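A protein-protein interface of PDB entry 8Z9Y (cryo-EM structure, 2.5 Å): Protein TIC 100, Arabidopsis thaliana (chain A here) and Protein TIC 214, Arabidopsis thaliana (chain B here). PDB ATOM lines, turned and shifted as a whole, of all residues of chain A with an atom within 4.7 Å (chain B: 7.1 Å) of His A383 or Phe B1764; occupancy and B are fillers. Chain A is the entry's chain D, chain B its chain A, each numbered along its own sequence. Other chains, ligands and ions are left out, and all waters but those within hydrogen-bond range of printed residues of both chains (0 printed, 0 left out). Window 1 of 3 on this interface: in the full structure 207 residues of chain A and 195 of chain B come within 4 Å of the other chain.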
ATOM      1  N   HIS A 255     -27.195 -36.039   4.562  1.00  0.00           N
ATOM      2  CA  HIS A 255     -28.549 -35.904   4.044  1.00  0.00           C
ATOM      3  C   HIS A 255     -28.570 -36.324   2.582  1.00  0.00           C
ATOM      4  O   HIS A 255     -27.657 -35.993   1.822  1.00  0.00           O
ATOM      5  CB  HIS A 255     -29.057 -34.464   4.184  1.00  0.00           C
ATOM      6  CG  HIS A 255     -29.346 -34.058   5.595  1.00  0.00           C
ATOM      7  ND1 HIS A 255     -28.465 -33.317   6.353  1.00  0.00           N
ATOM      8  CD2 HIS A 255     -30.420 -34.287   6.385  1.00  0.00           C
ATOM      9  CE1 HIS A 255     -28.983 -33.109   7.549  1.00  0.00           C
ATOM     10  NE2 HIS A 255     -30.169 -33.688   7.595  1.00  0.00           N
ATOM     11  N   GLY A 339     -34.018 -38.263   4.155  1.00  0.00           N
ATOM     12  CA  GLY A 339     -33.720 -37.967   5.541  1.00  0.00           C
ATOM     13  C   GLY A 339     -32.240 -37.982   5.859  1.00  0.00           C
ATOM     14  O   GLY A 339     -31.424 -37.490   5.076  1.00  0.00           O
ATOM     15  N   GLN A 340     -31.882 -38.544   7.009  1.00  0.00           N
ATOM     16  CA  GLN A 340     -30.500 -38.600   7.460  1.00  0.00           C
ATOM     17  C   GLN A 340     -29.918 -39.982   7.196  1.00  0.00           C
ATOM     18  O   GLN A 340     -30.609 -40.995   7.327  1.00  0.00           O
ATOM     19  CB  GLN A 340     -30.397 -38.265   8.947  1.00  0.00           C
ATOM     20  CG  GLN A 340     -30.712 -36.818   9.281  1.00  0.00           C
ATOM     21  CD  GLN A 340     -30.512 -36.503  10.748  1.00  0.00           C
ATOM     22  OE1 GLN A 340     -31.134 -37.113  11.616  1.00  0.00           O
ATOM     23  NE2 GLN A 340     -29.637 -35.547  11.034  1.00  0.00           N
ATOM     24  N   CYS A 349     -34.052 -38.946  11.730  1.00  0.00           N
ATOM     25  CA  CYS A 349     -35.420 -38.661  11.324  1.00  0.00           C
ATOM     26  C   CYS A 349     -35.497 -38.550   9.808  1.00  0.00           C
ATOM     27  O   CYS A 349     -34.629 -37.944   9.174  1.00  0.00           O
ATOM     28  CB  CYS A 349     -35.927 -37.370  11.971  1.00  0.00           C
ATOM     29  SG  CYS A 349     -35.320 -37.039  13.647  1.00  0.00           S
ATOM     30  N   ILE A 379     -39.875 -32.088  12.942  1.00  0.00           N
ATOM     31  CA  ILE A 379     -38.449 -32.355  12.785  1.00  0.00           C
ATOM     32  C   ILE A 379     -38.203 -33.243  11.571  1.00  0.00           C
ATOM     33  O   ILE A 379     -37.238 -33.044  10.820  1.00  0.00           O
ATOM     34  CB  ILE A 379     -37.886 -32.975  14.075  1.00  0.00           C
ATOM     35  CG1 ILE A 379     -37.942 -31.955  15.214  1.00  0.00           C
ATOM     36  CG2 ILE A 379     -36.462 -33.453  13.867  1.00  0.00           C
ATOM     37  CD1 ILE A 379     -37.541 -32.518  16.554  1.00  0.00           C
ATOM     38  N   CYS A 380     -39.074 -34.231  11.355  1.00  0.00           N
ATOM     39  CA  CYS A 380     -38.950 -35.080  10.175  1.00  0.00           C
ATOM     40  C   CYS A 380     -39.118 -34.270   8.898  1.00  0.00           C
ATOM     41  O   CYS A 380     -38.393 -34.485   7.921  1.00  0.00           O
ATOM     42  CB  CYS A 380     -39.973 -36.213  10.232  1.00  0.00           C
ATOM     43  SG  CYS A 380     -39.554 -37.537  11.383  1.00  0.00           S
ATOM     44  N   ALA A 381     -40.070 -33.335   8.883  1.00  0.00           N
ATOM     45  CA  ALA A 381     -40.248 -32.480   7.714  1.00  0.00           C
ATOM     46  C   ALA A 381     -39.023 -31.606   7.477  1.00  0.00           C
ATOM     47  O   ALA A 381     -38.594 -31.421   6.331  1.00  0.00           O
ATOM     48  CB  ALA A 381     -41.498 -31.619   7.879  1.00  0.00           C
ATOM     49  N   LEU A 382     -38.449 -31.059   8.550  1.00  0.00           N
ATOM     50  CA  LEU A 382     -37.251 -30.237   8.413  1.00  0.00           C
ATOM     51  C   LEU A 382     -36.098 -31.042   7.825  1.00  0.00           C
ATOM     52  O   LEU A 382     -35.396 -30.580   6.916  1.00  0.00           O
ATOM     53  CB  LEU A 382     -36.863 -29.652   9.769  1.00  0.00           C
ATOM     54  CG  LEU A 382     -35.455 -29.066   9.871  1.00  0.00           C
ATOM     55  CD1 LEU A 382     -35.416 -27.663   9.288  1.00  0.00           C
ATOM     56  CD2 LEU A 382     -34.974 -29.068  11.312  1.00  0.00           C
ATOM     57  N   HIS A 383     -35.894 -32.260   8.329  1.00  0.00           N
ATOM     58  CA  HIS A 383     -34.799 -33.080   7.821  1.00  0.00           C
ATOM     59  C   HIS A 383     -35.061 -33.548   6.396  1.00  0.00           C
ATOM     60  O   HIS A 383     -34.120 -33.665   5.604  1.00  0.00           O
ATOM     61  CB  HIS A 383     -34.557 -34.267   8.748  1.00  0.00           C
ATOM     62  CG  HIS A 383     -33.758 -33.920   9.964  1.00  0.00           C
ATOM     63  ND1 HIS A 383     -32.403 -33.674   9.920  1.00  0.00           N
ATOM     64  CD2 HIS A 383     -34.126 -33.766  11.258  1.00  0.00           C
ATOM     65  CE1 HIS A 383     -31.969 -33.388  11.134  1.00  0.00           C
ATOM     66  NE2 HIS A 383     -32.995 -33.438  11.965  1.00  0.00           N
ATOM     67  N   SER A 384     -36.322 -33.805   6.045  1.00  0.00           N
ATOM     68  CA  SER A 384     -36.652 -34.143   4.665  1.00  0.00           C
ATOM     69  C   SER A 384     -36.353 -32.980   3.727  1.00  0.00           C
ATOM     70  O   SER A 384     -35.824 -33.180   2.628  1.00  0.00           O
ATOM     71  CB  SER A 384     -38.119 -34.552   4.564  1.00  0.00           C
ATOM     72  OG  SER A 384     -38.418 -35.055   3.276  1.00  0.00           O
ATOM     73  N   GLY A 385     -36.690 -31.758   4.142  1.00  0.00           N
ATOM     74  CA  GLY A 385     -36.361 -30.598   3.328  1.00  0.00           C
ATOM     75  C   GLY A 385     -34.865 -30.404   3.176  1.00  0.00           C
ATOM     76  O   GLY A 385     -34.376 -30.073   2.090  1.00  0.00           O
ATOM     77  N   LEU A 386     -34.116 -30.613   4.262  1.00  0.00           N
ATOM     78  CA  LEU A 386     -32.662 -30.540   4.175  1.00  0.00           C
ATOM     79  C   LEU A 386     -32.116 -31.586   3.211  1.00  0.00           C
ATOM     80  O   LEU A 386     -31.210 -31.300   2.420  1.00  0.00           O
ATOM     81  CB  LEU A 386     -32.042 -30.714   5.561  1.00  0.00           C
ATOM     82  CG  LEU A 386     -32.048 -29.484   6.471  1.00  0.00           C
ATOM     83  CD1 LEU A 386     -31.600 -29.857   7.872  1.00  0.00           C
ATOM     84  CD2 LEU A 386     -31.161 -28.395   5.897  1.00  0.00           C
ATOM     85  N   ALA A 387     -32.654 -32.807   3.264  1.00  0.00           N
ATOM     86  CA  ALA A 387     -32.208 -33.857   2.355  1.00  0.00           C
ATOM     87  C   ALA A 387     -32.520 -33.506   0.906  1.00  0.00           C
ATOM     88  O   ALA A 387     -31.706 -33.759   0.011  1.00  0.00           O
ATOM     89  CB  ALA A 387     -32.854 -35.188   2.734  1.00  0.00           C
ATOM     90  N   ASP B1292     -29.327 -32.561  22.059  1.00  0.00           N
ATOM     91  CA  ASP B1292     -29.546 -32.685  20.620  1.00  0.00           C
ATOM     92  C   ASP B1292     -31.001 -32.422  20.249  1.00  0.00           C
ATOM     93  O   ASP B1292     -31.282 -31.781  19.227  1.00  0.00           O
ATOM     94  CB  ASP B1292     -29.111 -34.071  20.145  1.00  0.00           C
ATOM     95  CG  ASP B1292     -28.934 -34.141  18.642  1.00  0.00           C
ATOM     96  OD1 ASP B1292     -28.714 -33.081  18.018  1.00  0.00           O
ATOM     97  OD2 ASP B1292     -29.011 -35.256  18.085  1.00  0.00           O
ATOM     98  N   TYR B1295     -31.553 -28.792  20.321  1.00  0.00           N
ATOM     99  CA  TYR B1295     -30.987 -28.181  19.122  1.00  0.00           C
ATOM    100  C   TYR B1295     -31.902 -28.361  17.916  1.00  0.00           C
ATOM    101  O   TYR B1295     -32.092 -27.427  17.127  1.00  0.00           O
ATOM    102  CB  TYR B1295     -29.606 -28.767  18.833  1.00  0.00           C
ATOM    103  CG  TYR B1295     -28.880 -28.075  17.703  1.00  0.00           C
ATOM    104  CD1 TYR B1295     -28.339 -26.809  17.872  1.00  0.00           C
ATOM    105  CD2 TYR B1295     -28.743 -28.685  16.463  1.00  0.00           C
ATOM    106  CE1 TYR B1295     -27.678 -26.172  16.842  1.00  0.00           C
ATOM    107  CE2 TYR B1295     -28.083 -28.057  15.428  1.00  0.00           C
ATOM    108  CZ  TYR B1295     -27.553 -26.801  15.622  1.00  0.00           C
ATOM    109  OH  TYR B1295     -26.895 -26.171  14.592  1.00  0.00           O
ATOM    110  N   ASN B1296     -32.467 -29.559  17.749  1.00  0.00           N
ATOM    111  CA  ASN B1296     -33.377 -29.796  16.631  1.00  0.00           C
ATOM    112  C   ASN B1296     -34.608 -28.901  16.722  1.00  0.00           C
ATOM    113  O   ASN B1296     -35.043 -28.317  15.718  1.00  0.00           O
ATOM    114  CB  ASN B1296     -33.789 -31.268  16.594  1.00  0.00           C
ATOM    115  CG  ASN B1296     -32.952 -32.084  15.631  1.00  0.00           C
ATOM    116  OD1 ASN B1296     -32.374 -31.548  14.688  1.00  0.00           O
ATOM    117  ND2 ASN B1296     -32.884 -33.387  15.867  1.00  0.00           N
ATOM    118  N   CYS B1299     -33.656 -25.387  15.758  1.00  0.00           N
ATOM    119  CA  CYS B1299     -33.533 -25.235  14.311  1.00  0.00           C
ATOM    120  C   CYS B1299     -34.902 -25.107  13.654  1.00  0.00           C
ATOM    121  O   CYS B1299     -35.133 -24.207  12.834  1.00  0.00           O
ATOM    122  CB  CYS B1299     -32.766 -26.418  13.720  1.00  0.00           C
ATOM    123  SG  CYS B1299     -31.070 -26.589  14.303  1.00  0.00           S
ATOM    124  N   PHE B1746     -43.614 -28.688   2.276  1.00  0.00           N
ATOM    125  CA  PHE B1746     -42.706 -27.946   3.144  1.00  0.00           C
ATOM    126  C   PHE B1746     -41.884 -26.920   2.373  1.00  0.00           C
ATOM    127  O   PHE B1746     -41.553 -25.862   2.918  1.00  0.00           O
ATOM    128  CB  PHE B1746     -41.785 -28.917   3.881  1.00  0.00           C
ATOM    129  CG  PHE B1746     -41.055 -28.304   5.038  1.00  0.00           C
ATOM    130  CD1 PHE B1746     -41.751 -27.769   6.108  1.00  0.00           C
ATOM    131  CD2 PHE B1746     -39.672 -28.267   5.061  1.00  0.00           C
ATOM    132  CE1 PHE B1746     -41.082 -27.208   7.176  1.00  0.00           C
ATOM    133  CE2 PHE B1746     -38.997 -27.705   6.126  1.00  0.00           C
ATOM    134  CZ  PHE B1746     -39.704 -27.175   7.185  1.00  0.00           C
ATOM    135  N   LEU B1756     -32.927 -23.252   3.974  1.00  0.00           N
ATOM    136  CA  LEU B1756     -32.447 -24.625   4.065  1.00  0.00           C
ATOM    137  C   LEU B1756     -31.052 -24.765   3.475  1.00  0.00           C
ATOM    138  O   LEU B1756     -30.234 -25.531   3.991  1.00  0.00           O
ATOM    139  CB  LEU B1756     -33.426 -25.569   3.368  1.00  0.00           C
ATOM    140  CG  LEU B1756     -34.686 -25.920   4.157  1.00  0.00           C
ATOM    141  CD1 LEU B1756     -35.550 -26.893   3.379  1.00  0.00           C
ATOM    142  CD2 LEU B1756     -34.313 -26.504   5.506  1.00  0.00           C
ATOM    143  N   CYS B1758     -28.731 -22.413   3.498  1.00  0.00           N
ATOM    144  CA  CYS B1758     -27.824 -21.864   4.503  1.00  0.00           C
ATOM    145  C   CYS B1758     -27.627 -22.834   5.663  1.00  0.00           C
ATOM    146  O   CYS B1758     -26.499 -23.029   6.137  1.00  0.00           O
ATOM    147  CB  CYS B1758     -28.352 -20.522   5.009  1.00  0.00           C
ATOM    148  SG  CYS B1758     -27.128 -19.534   5.897  1.00  0.00           S
ATOM    149  N   MET B1759     -28.714 -23.456   6.131  1.00  0.00           N
ATOM    150  CA  MET B1759     -28.600 -24.415   7.228  1.00  0.00           C
ATOM    151  C   MET B1759     -27.748 -25.614   6.831  1.00  0.00           C
ATOM    152  O   MET B1759     -26.918 -26.081   7.617  1.00  0.00           O
ATOM    153  CB  MET B1759     -29.985 -24.872   7.683  1.00  0.00           C
ATOM    154  CG  MET B1759     -30.881 -23.755   8.184  1.00  0.00           C
ATOM    155  SD  MET B1759     -32.092 -24.321   9.391  1.00  0.00           S
ATOM    156  CE  MET B1759     -32.511 -22.776  10.192  1.00  0.00           C
ATOM    157  N   ASN B1760     -27.939 -26.127   5.616  1.00  0.00           N
ATOM    158  CA  ASN B1760     -27.121 -27.242   5.156  1.00  0.00           C
ATOM    159  C   ASN B1760     -25.657 -26.837   5.052  1.00  0.00           C
ATOM    160  O   ASN B1760     -24.760 -27.650   5.302  1.00  0.00           O
ATOM    161  CB  ASN B1760     -27.634 -27.752   3.812  1.00  0.00           C
ATOM    162  CG  ASN B1760     -27.260 -29.195   3.559  1.00  0.00           C
ATOM    163  OD1 ASN B1760     -27.269 -30.020   4.472  1.00  0.00           O
ATOM    164  ND2 ASN B1760     -26.924 -29.509   2.315  1.00  0.00           N
ATOM    165  N   ARG B1761     -25.397 -25.583   4.679  1.00  0.00           N
ATOM    166  CA  ARG B1761     -24.020 -25.110   4.605  1.00  0.00           C
ATOM    167  C   ARG B1761     -23.374 -25.049   5.985  1.00  0.00           C
ATOM    168  O   ARG B1761     -22.244 -25.516   6.170  1.00  0.00           O
ATOM    169  CB  ARG B1761     -23.965 -23.733   3.940  1.00  0.00           C
ATOM    170  CG  ARG B1761     -24.355 -23.738   2.471  1.00  0.00           C
ATOM    171  CD  ARG B1761     -24.254 -22.379   1.797  1.00  0.00           C
ATOM    172  NE  ARG B1761     -24.704 -22.420   0.409  1.00  0.00           N
ATOM    173  CZ  ARG B1761     -24.827 -21.353  -0.366  1.00  0.00           C
ATOM    174  NH1 ARG B1761     -24.528 -20.149   0.106  1.00  0.00           N
ATOM    175  NH2 ARG B1761     -25.245 -21.484  -1.619  1.00  0.00           N
ATOM    176  N   TYR B1762     -24.073 -24.481   6.971  1.00  0.00           N
ATOM    177  CA  TYR B1762     -23.414 -24.067   8.204  1.00  0.00           C
ATOM    178  C   TYR B1762     -23.976 -24.659   9.491  1.00  0.00           C
ATOM    179  O   TYR B1762     -23.453 -24.342  10.565  1.00  0.00           O
ATOM    180  CB  TYR B1762     -23.444 -22.536   8.320  1.00  0.00           C
ATOM    181  CG  TYR B1762     -22.454 -21.834   7.423  1.00  0.00           C
ATOM    182  CD1 TYR B1762     -21.092 -21.900   7.676  1.00  0.00           C
ATOM    183  CD2 TYR B1762     -22.881 -21.104   6.324  1.00  0.00           C
ATOM    184  CE1 TYR B1762     -20.183 -21.260   6.860  1.00  0.00           C
ATOM    185  CE2 TYR B1762     -21.981 -20.461   5.501  1.00  0.00           C
ATOM    186  CZ  TYR B1762     -20.633 -20.541   5.774  1.00  0.00           C
ATOM    187  OH  TYR B1762     -19.732 -19.901   4.957  1.00  0.00           O
ATOM    188  N   TRP B1763     -25.011 -25.499   9.438  1.00  0.00           N
ATOM    189  CA  TRP B1763     -25.664 -25.923  10.670  1.00  0.00           C
ATOM    190  C   TRP B1763     -25.532 -27.404  10.990  1.00  0.00           C
ATOM    191  O   TRP B1763     -25.761 -27.785  12.141  1.00  0.00           O
ATOM    192  CB  TRP B1763     -27.157 -25.560  10.637  1.00  0.00           C
ATOM    193  CG  TRP B1763     -27.422 -24.112  10.899  1.00  0.00           C
ATOM    194  CD1 TRP B1763     -26.797 -23.049  10.320  1.00  0.00           C
ATOM    195  CD2 TRP B1763     -28.382 -23.566  11.808  1.00  0.00           C
ATOM    196  NE1 TRP B1763     -27.308 -21.873  10.811  1.00  0.00           N
ATOM    197  CE2 TRP B1763     -28.283 -22.164  11.727  1.00  0.00           C
ATOM    198  CE3 TRP B1763     -29.317 -24.126  12.681  1.00  0.00           C
ATOM    199  CZ2 TRP B1763     -29.084 -21.315  12.485  1.00  0.00           C
ATOM    200  CZ3 TRP B1763     -30.109 -23.281  13.434  1.00  0.00           C
ATOM    201  CH2 TRP B1763     -29.988 -21.891  13.331  1.00  0.00           C
ATOM    202  N   PHE B1764     -25.177 -28.248  10.024  1.00  0.00           N
ATOM    203  CA  PHE B1764     -25.115 -29.685  10.253  1.00  0.00           C
ATOM    204  C   PHE B1764     -23.845 -30.271   9.658  1.00  0.00           C
ATOM    205  O   PHE B1764     -23.468 -29.941   8.530  1.00  0.00           O
ATOM    206  CB  PHE B1764     -26.334 -30.394   9.657  1.00  0.00           C
ATOM    207  CG  PHE B1764     -27.584 -30.235  10.471  1.00  0.00           C
ATOM    208  CD1 PHE B1764     -27.858 -31.100  11.515  1.00  0.00           C
ATOM    209  CD2 PHE B1764     -28.483 -29.221  10.194  1.00  0.00           C
ATOM    210  CE1 PHE B1764     -29.005 -30.958  12.266  1.00  0.00           C
ATOM    211  CE2 PHE B1764     -29.632 -29.074  10.943  1.00  0.00           C
ATOM    212  CZ  PHE B1764     -29.894 -29.944  11.980  1.00  0.00           C
ATOM    213  N   ASN B1765     -23.198 -31.151  10.426  1.00  0.00           N
ATOM    214  CA  ASN B1765     -22.026 -31.902   9.970  1.00  0.00           C
ATOM    215  C   ASN B1765     -20.944 -30.975   9.425  1.00  0.00           C
ATOM    216  O   ASN B1765     -20.301 -31.259   8.412  1.00  0.00           O
ATOM    217  CB  ASN B1765     -22.423 -32.948   8.927  1.00  0.00           C
ATOM    218  CG  ASN B1765     -23.359 -34.000   9.484  1.00  0.00           C
ATOM    219  OD1 ASN B1765     -23.034 -34.686  10.452  1.00  0.00           O
ATOM    220  ND2 ASN B1765     -24.529 -34.132   8.873  1.00  0.00           N
ATOM    221  N   THR B1766     -20.739 -29.852  10.107  1.00  0.00           N
ATOM    222  CA  THR B1766     -19.817 -28.828   9.640  1.00  0.00           C
ATOM    223  C   THR B1766     -18.371 -29.079  10.046  1.00  0.00           C
ATOM    224  O   THR B1766     -17.487 -28.338   9.603  1.00  0.00           O
ATOM    225  CB  THR B1766     -20.257 -27.454  10.156  1.00  0.00           C
ATOM    226  OG1 THR B1766     -19.449 -26.436   9.557  1.00  0.00           O
ATOM    227  CG2 THR B1766     -20.117 -27.381  11.666  1.00  0.00           C
ATOM    228  N   THR B1767     -18.101 -30.096  10.871  1.00  0.00           N
ATOM    229  CA  THR B1767     -16.747 -30.365  11.337  1.00  0.00           C
ATOM    230  C   THR B1767     -16.352 -31.832  11.218  1.00  0.00           C
ATOM    231  O   THR B1767     -15.310 -32.222  11.757  1.00  0.00           O
ATOM    232  CB  THR B1767     -16.570 -29.920  12.796  1.00  0.00           C
ATOM    233  OG1 THR B1767     -17.460 -30.665  13.637  1.00  0.00           O
ATOM    234  CG2 THR B1767     -16.848 -28.433  12.954  1.00  0.00           C
ATOM    235  N   ASN B1768     -17.140 -32.655  10.531  1.00  0.00           N
ATOM    236  CA  ASN B1768     -16.898 -34.090  10.479  1.00  0.00           C
ATOM    237  C   ASN B1768     -16.190 -34.532   9.204  1.00  0.00           C
ATOM    238  O   ASN B1768     -16.078 -35.736   8.956  1.00  0.00           O
ATOM    239  CB  ASN B1768     -18.217 -34.851  10.636  1.00  0.00           C
ATOM    240  CG  ASN B1768     -19.003 -34.928   9.345  1.00  0.00           C
ATOM    241  OD1 ASN B1768     -19.121 -33.943   8.616  1.00  0.00           O
ATOM    242  ND2 ASN B1768     -19.549 -36.102   9.055  1.00  0.00           N
ATOM    243  N   ASN B1770     -17.146 -33.582   6.025  1.00  0.00           N
ATOM    244  CA  ASN B1770     -18.064 -33.638   4.896  1.00  0.00           C
ATOM    245  C   ASN B1770     -18.190 -32.314   4.159  1.00  0.00           C
ATOM    246  O   ASN B1770     -18.460 -32.313   2.955  1.00  0.00           O
ATOM    247  CB  ASN B1770     -19.453 -34.080   5.368  1.00  0.00           C
ATOM    248  CG  ASN B1770     -20.152 -34.968   4.364  1.00  0.00           C
ATOM    249  OD1 ASN B1770     -20.046 -34.759   3.156  1.00  0.00           O
ATOM    250  ND2 ASN B1770     -20.875 -35.966   4.857  1.00  0.00           N
ATOM    251  N   HIS B1771     -18.001 -31.191   4.847  1.00  0.00           N
ATOM    252  CA  HIS B1771     -18.142 -29.870   4.254  1.00  0.00           C
ATOM    253  C   HIS B1771     -16.833 -29.102   4.368  1.00  0.00           C
ATOM    254  O   HIS B1771     -16.131 -29.197   5.378  1.00  0.00           O
ATOM    255  CB  HIS B1771     -19.265 -29.075   4.929  1.00  0.00           C
ATOM    256  CG  HIS B1771     -20.608 -29.731   4.840  1.00  0.00           C
ATOM    257  ND1 HIS B1771     -20.939 -30.852   5.570  1.00  0.00           N
ATOM    258  CD2 HIS B1771     -21.703 -29.421   4.109  1.00  0.00           C
ATOM    259  CE1 HIS B1771     -22.181 -31.204   5.292  1.00  0.00           C
ATOM    260  NE2 HIS B1771     -22.667 -30.353   4.407  1.00  0.00           N
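The side-chain amide oxygen (OD1) of Asn B1296 sits at hydrogen-bond distance from a ring nitrogen (NE2) of His A383 (3.4 Å).
A ring nitrogen (ND1) of His A383 sits at hydrogen-bond distance from a ring nitrogen (NE2) of His A255, at 3.2 Å.
Among the printed residues, pairs that only touch across the chains: His A255 with Asn B1760 (3.98 Å), Ile A379 with Asn B1296 (3.95 Å), Ala A381 with Phe B1746 (3.6 Å), Leu A382 with Phe B1746 (3.8 Å), His A383 with Phe B1764 (3.996 Å), Gly A385 with Leu B1756 (3.6 Å), Leu A386 with Leu B1756 (3.6 Å), Leu A386 with Asn B1760 (3.95 Å) and Leu A386 with Phe B1764 (3.7 Å).
Cys A349 touches none of the printed residues of chain B. Of the printed residues of chain B, Leu A382 touches Phe B1746 (3.8 Å). Printed residues of chain B within 4 Å of His A383: Asn B1296 (3.4 Å) and Phe B1764 (3.996 Å). Of the printed residues of chain B, Gly A385 touches Leu B1756 (3.6 Å). Ala A387 touches none of the printed residues of chain B. Printed residues of chain A within 4 Å of Asn B1296: Ile A379 and His A383. Of the printed residues of chain A, Leu B1756 touches Gly A385 (3.6 Å) and Leu A386 (3.6 Å). Printed residues of chain A within 4 Å of Asn B1760: His A255 and Leu A386. Of the printed residues of chain A, Phe B1764 touches His A383 (3.996 Å) and Leu A386 (3.7 Å). The nearest printed residue of chain B that does not touch His A255 is Phe B1764 (4.3 Å).
Of the 13 printed residues of chain A, 7 touch a printed residue of chain B. Among the printed residues, 10 pairs touch across the chains. Among the printed residues, no Asp or Glu carboxylate lies within 4 Å of a Lys or Arg side-chain nitrogen of the other chain.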
